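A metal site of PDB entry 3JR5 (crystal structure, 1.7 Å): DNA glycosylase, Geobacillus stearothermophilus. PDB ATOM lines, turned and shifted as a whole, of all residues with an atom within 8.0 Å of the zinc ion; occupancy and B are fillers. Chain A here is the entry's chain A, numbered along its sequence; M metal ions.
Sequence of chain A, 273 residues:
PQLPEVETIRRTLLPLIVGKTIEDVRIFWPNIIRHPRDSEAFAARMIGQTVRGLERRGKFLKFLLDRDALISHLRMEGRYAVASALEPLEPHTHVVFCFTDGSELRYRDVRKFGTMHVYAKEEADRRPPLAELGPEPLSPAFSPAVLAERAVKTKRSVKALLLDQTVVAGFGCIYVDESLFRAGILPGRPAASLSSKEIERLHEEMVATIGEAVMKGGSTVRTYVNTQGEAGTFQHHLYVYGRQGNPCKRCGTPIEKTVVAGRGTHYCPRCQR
OG1 of Thr 253 lies close to SG of Cys 251. The backbone NH (N) of Arg 250 lies close to the side-chain sulfur (SG) of Cys 248, at 3.4 Å. The backbone NH (N) of Cys 248 sits at hydrogen-bond distance from the backbone carbonyl oxygen (O) of Thr 253 (2.7 Å). The side-chain sulfur of Cys 268 sits close to the backbone NH of Arg 270, 3.4 Å away. The backbone NH (N) of Cys 268 is in hydrogen-bond range of the side-chain amide oxygen (OE1) of Gln 272 (2.9 Å).
Within 4 Å of the zinc ion: Cys 248, Cys 251, Cys 268 and Cys 271.
The zinc ion is bound by the side-chain sulfur (SG) of Cys 271 (2.3 Å), the side-chain sulfur (SG) of Cys 251 (2.3 Å), the side-chain sulfur (SG) of Cys 248 (2.4 Å) and the side-chain sulfur (SG) of Cys 268 (2.4 Å). The zinc ion has four donor atoms within binding distance.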
ATOM      1  N   PHE A 181      -1.694 -14.414  19.243  1.00  0.00           N
ATOM      2  CA  PHE A 181      -1.669 -12.949  19.398  1.00  0.00           C
ATOM      3  C   PHE A 181      -2.715 -12.480  20.421  1.00  0.00           C
ATOM      4  O   PHE A 181      -2.424 -11.686  21.340  1.00  0.00           O
ATOM      5  CB  PHE A 181      -1.917 -12.219  18.080  1.00  0.00           C
ATOM      6  CG  PHE A 181      -2.120 -10.740  18.264  1.00  0.00           C
ATOM      7  CD1 PHE A 181      -1.025  -9.882  18.323  1.00  0.00           C
ATOM      8  CD2 PHE A 181      -3.393 -10.208  18.420  1.00  0.00           C
ATOM      9  CE1 PHE A 181      -1.195  -8.516  18.506  1.00  0.00           C
ATOM     10  CE2 PHE A 181      -3.590  -8.852  18.616  1.00  0.00           C
ATOM     11  CZ  PHE A 181      -2.476  -7.990  18.663  1.00  0.00           C
ATOM     12  N   TYR A 239      -5.349  -9.842  13.089  1.00  0.00           N
ATOM     13  CA  TYR A 239      -4.374  -8.967  13.763  1.00  0.00           C
ATOM     14  C   TYR A 239      -2.954  -9.136  13.254  1.00  0.00           C
ATOM     15  O   TYR A 239      -2.182  -8.155  13.197  1.00  0.00           O
ATOM     16  CB  TYR A 239      -4.371  -9.230  15.263  1.00  0.00           C
ATOM     17  CG  TYR A 239      -5.616  -8.751  15.978  1.00  0.00           C
ATOM     18  CD1 TYR A 239      -5.786  -7.415  16.304  1.00  0.00           C
ATOM     19  CD2 TYR A 239      -6.611  -9.654  16.328  1.00  0.00           C
ATOM     20  CE1 TYR A 239      -6.926  -6.990  16.967  1.00  0.00           C
ATOM     21  CE2 TYR A 239      -7.764  -9.233  16.979  1.00  0.00           C
ATOM     22  CZ  TYR A 239      -7.907  -7.887  17.292  1.00  0.00           C
ATOM     23  OH  TYR A 239      -9.030  -7.452  17.952  1.00  0.00           O
ATOM     24  N   VAL A 240      -2.590 -10.367  12.909  1.00  0.00           N
ATOM     25  CA  VAL A 240      -1.200 -10.655  12.536  1.00  0.00           C
ATOM     26  C   VAL A 240      -1.004 -11.408  11.223  1.00  0.00           C
ATOM     27  O   VAL A 240      -0.047 -11.121  10.487  1.00  0.00           O
ATOM     28  CB  VAL A 240      -0.399 -11.355  13.691  1.00  0.00           C
ATOM     29  CG1 VAL A 240      -0.311 -10.451  14.923  1.00  0.00           C
ATOM     30  CG2 VAL A 240      -1.007 -12.714  14.067  1.00  0.00           C
ATOM     31  N   PRO A 247       1.717  -1.960  10.887  1.00  0.00           N
ATOM     32  CA  PRO A 247       1.631  -1.700  12.329  1.00  0.00           C
ATOM     33  C   PRO A 247       0.642  -2.643  13.004  1.00  0.00           C
ATOM     34  O   PRO A 247      -0.431  -2.916  12.461  1.00  0.00           O
ATOM     35  CB  PRO A 247       1.073  -0.263  12.393  1.00  0.00           C
ATOM     36  CG  PRO A 247       1.278   0.310  11.032  1.00  0.00           C
ATOM     37  CD  PRO A 247       1.195  -0.839  10.080  1.00  0.00           C
ATOM     38  N   CYS A 248       0.983  -3.114  14.200  1.00  0.00           N
ATOM     39  CA  CYS A 248       0.026  -3.818  15.038  1.00  0.00           C
ATOM     40  C   CYS A 248      -1.213  -2.928  15.261  1.00  0.00           C
ATOM     41  O   CYS A 248      -1.082  -1.719  15.467  1.00  0.00           O
ATOM     42  CB  CYS A 248       0.689  -4.193  16.358  1.00  0.00           C
ATOM     43  SG  CYS A 248      -0.425  -4.986  17.557  1.00  0.00           S
ATOM     44  N   LYS A 249      -2.406  -3.526  15.201  1.00  0.00           N
ATOM     45  CA  LYS A 249      -3.659  -2.788  15.366  1.00  0.00           C
ATOM     46  C   LYS A 249      -3.878  -2.330  16.803  1.00  0.00           C
ATOM     47  O   LYS A 249      -4.689  -1.429  17.061  1.00  0.00           O
ATOM     48  CB  LYS A 249      -4.858  -3.659  14.937  1.00  0.00           C
ATOM     49  CG  LYS A 249      -4.899  -4.015  13.462  1.00  0.00           C
ATOM     50  CD  LYS A 249      -6.200  -4.764  13.125  1.00  0.00           C
ATOM     51  CE  LYS A 249      -6.268  -5.147  11.662  1.00  0.00           C
ATOM     52  NZ  LYS A 249      -7.590  -5.814  11.351  1.00  0.00           N
ATOM     53  N   ARG A 250      -3.162  -2.964  17.735  1.00  0.00           N
ATOM     54  CA  ARG A 250      -3.301  -2.646  19.150  1.00  0.00           C
ATOM     55  C   ARG A 250      -2.186  -1.737  19.683  1.00  0.00           C
ATOM     56  O   ARG A 250      -2.459  -0.881  20.526  1.00  0.00           O
ATOM     57  CB  ARG A 250      -3.375  -3.927  19.991  1.00  0.00           C
ATOM     58  CG  ARG A 250      -4.603  -4.771  19.673  1.00  0.00           C
ATOM     59  CD  ARG A 250      -4.957  -5.675  20.836  1.00  0.00           C
ATOM     60  NE  ARG A 250      -6.262  -6.304  20.662  1.00  0.00           N
ATOM     61  CZ  ARG A 250      -6.635  -7.429  21.259  1.00  0.00           C
ATOM     62  NH1 ARG A 250      -5.785  -8.052  22.064  1.00  0.00           N
ATOM     63  NH2 ARG A 250      -7.838  -7.925  21.041  1.00  0.00           N
ATOM     64  N   CYS A 251      -0.947  -1.908  19.210  1.00  0.00           N
ATOM     65  CA  CYS A 251       0.168  -1.129  19.770  1.00  0.00           C
ATOM     66  C   CYS A 251       0.995  -0.351  18.744  1.00  0.00           C
ATOM     67  O   CYS A 251       1.817   0.494  19.111  1.00  0.00           O
ATOM     68  CB  CYS A 251       1.088  -2.010  20.619  1.00  0.00           C
ATOM     69  SG  CYS A 251       2.154  -3.105  19.650  1.00  0.00           S
ATOM     70  N   GLY A 252       0.792  -0.667  17.465  1.00  0.00           N
ATOM     71  CA  GLY A 252       1.479   0.028  16.380  1.00  0.00           C
ATOM     72  C   GLY A 252       2.869  -0.448  16.039  1.00  0.00           C
ATOM     73  O   GLY A 252       3.506   0.070  15.114  1.00  0.00           O
ATOM     74  N   THR A 253       3.372  -1.419  16.787  1.00  0.00           N
ATOM     75  CA  THR A 253       4.686  -2.018  16.515  1.00  0.00           C
ATOM     76  C   THR A 253       4.569  -2.817  15.217  1.00  0.00           C
ATOM     77  O   THR A 253       3.571  -3.514  15.006  1.00  0.00           O
ATOM     78  CB  THR A 253       5.078  -2.968  17.657  1.00  0.00           C
ATOM     79  OG1 THR A 253       5.121  -2.242  18.903  1.00  0.00           O
ATOM     80  CG2 THR A 253       6.455  -3.627  17.401  1.00  0.00           C
ATOM     81  N   PRO A 254       5.593  -2.732  14.326  1.00  0.00           N
ATOM     82  CA  PRO A 254       5.485  -3.541  13.099  1.00  0.00           C
ATOM     83  C   PRO A 254       5.377  -5.036  13.378  1.00  0.00           C
ATOM     84  O   PRO A 254       6.138  -5.603  14.149  1.00  0.00           O
ATOM     85  CB  PRO A 254       6.795  -3.235  12.350  1.00  0.00           C
ATOM     86  CG  PRO A 254       7.208  -1.853  12.878  1.00  0.00           C
ATOM     87  CD  PRO A 254       6.773  -1.857  14.329  1.00  0.00           C
ATOM     88  N   ILE A 255       4.414  -5.686  12.723  1.00  0.00           N
ATOM     89  CA  ILE A 255       4.261  -7.133  12.812  1.00  0.00           C
ATOM     90  C   ILE A 255       5.470  -7.821  12.172  1.00  0.00           C
ATOM     91  O   ILE A 255       6.002  -7.359  11.153  1.00  0.00           O
ATOM     92  CB  ILE A 255       2.934  -7.557  12.147  1.00  0.00           C
ATOM     93  CG1 ILE A 255       1.757  -6.941  12.906  1.00  0.00           C
ATOM     94  CG2 ILE A 255       2.794  -9.086  12.111  1.00  0.00           C
ATOM     95  CD1 ILE A 255       1.768  -7.206  14.433  1.00  0.00           C
ATOM     96  N   TYR A 267       3.634 -12.498  14.203  1.00  0.00           N
ATOM     97  CA  TYR A 267       3.436 -12.145  15.606  1.00  0.00           C
ATOM     98  C   TYR A 267       3.777 -10.674  15.873  1.00  0.00           C
ATOM     99  O   TYR A 267       4.517 -10.053  15.120  1.00  0.00           O
ATOM    100  CB  TYR A 267       4.263 -13.062  16.534  1.00  0.00           C
ATOM    101  CG  TYR A 267       5.746 -12.925  16.307  1.00  0.00           C
ATOM    102  CD1 TYR A 267       6.525 -12.108  17.128  1.00  0.00           C
ATOM    103  CD2 TYR A 267       6.376 -13.597  15.264  1.00  0.00           C
ATOM    104  CE1 TYR A 267       7.885 -11.978  16.918  1.00  0.00           C
ATOM    105  CE2 TYR A 267       7.747 -13.467  15.043  1.00  0.00           C
ATOM    106  CZ  TYR A 267       8.485 -12.659  15.874  1.00  0.00           C
ATOM    107  OH  TYR A 267       9.838 -12.516  15.665  1.00  0.00           O
ATOM    108  N   CYS A 268       3.221 -10.115  16.948  1.00  0.00           N
ATOM    109  CA  CYS A 268       3.660  -8.809  17.436  1.00  0.00           C
ATOM    110  C   CYS A 268       4.652  -9.004  18.578  1.00  0.00           C
ATOM    111  O   CYS A 268       4.313  -9.611  19.590  1.00  0.00           O
ATOM    112  CB  CYS A 268       2.459  -8.005  17.936  1.00  0.00           C
ATOM    113  SG  CYS A 268       3.019  -6.421  18.676  1.00  0.00           S
ATOM    114  N   PRO A 269       5.876  -8.468  18.430  1.00  0.00           N
ATOM    115  CA  PRO A 269       6.903  -8.724  19.450  1.00  0.00           C
ATOM    116  C   PRO A 269       6.660  -7.955  20.754  1.00  0.00           C
ATOM    117  O   PRO A 269       7.331  -8.217  21.753  1.00  0.00           O
ATOM    118  CB  PRO A 269       8.201  -8.252  18.782  1.00  0.00           C
ATOM    119  CG  PRO A 269       7.781  -7.258  17.751  1.00  0.00           C
ATOM    120  CD  PRO A 269       6.372  -7.649  17.306  1.00  0.00           C
ATOM    121  N   ARG A 270       5.701  -7.022  20.736  1.00  0.00           N
ATOM    122  CA  ARG A 270       5.343  -6.273  21.944  1.00  0.00           C
ATOM    123  C   ARG A 270       4.145  -6.867  22.681  1.00  0.00           C
ATOM    124  O   ARG A 270       4.199  -7.075  23.894  1.00  0.00           O
ATOM    125  CB  ARG A 270       5.054  -4.802  21.623  1.00  0.00           C
ATOM    126  CG  ARG A 270       4.771  -3.964  22.884  1.00  0.00           C
ATOM    127  CD  ARG A 270       4.598  -2.474  22.550  1.00  0.00           C
ATOM    128  NE  ARG A 270       4.297  -1.719  23.766  1.00  0.00           N
ATOM    129  CZ  ARG A 270       4.320  -0.390  23.854  1.00  0.00           C
ATOM    130  NH1 ARG A 270       4.058   0.183  25.018  1.00  0.00           N
ATOM    131  NH2 ARG A 270       4.624   0.351  22.780  1.00  0.00           N
ATOM    132  N   CYS A 271       3.069  -7.178  21.954  1.00  0.00           N
ATOM    133  CA  CYS A 271       1.851  -7.696  22.585  1.00  0.00           C
ATOM    134  C   CYS A 271       2.005  -9.150  23.050  1.00  0.00           C
ATOM    135  O   CYS A 271       1.299  -9.596  23.960  1.00  0.00           O
ATOM    136  CB  CYS A 271       0.653  -7.608  21.632  1.00  0.00           C
ATOM    137  SG  CYS A 271       0.061  -5.926  21.262  1.00  0.00           S
ATOM    138  N   GLN A 272       2.891  -9.894  22.405  1.00  0.00           N
ATOM    139  CA  GLN A 272       3.106 -11.300  22.728  1.00  0.00           C
ATOM    140  C   GLN A 272       4.378 -11.504  23.530  1.00  0.00           C
ATOM    141  O   GLN A 272       5.426 -10.932  23.208  1.00  0.00           O
ATOM    142  CB  GLN A 272       3.093 -12.149  21.437  1.00  0.00           C
ATOM    143  CG  GLN A 272       1.706 -12.138  20.781  1.00  0.00           C
ATOM    144  CD  GLN A 272       1.702 -12.727  19.375  1.00  0.00           C
ATOM    145  OE1 GLN A 272       1.627 -11.994  18.387  1.00  0.00           O
ATOM    146  NE2 GLN A 272       1.764 -14.064  19.272  1.00  0.00           N
HETATM  147 ZN    ZN M   1       1.110  -5.174  19.339  1.00  0.00          ZN
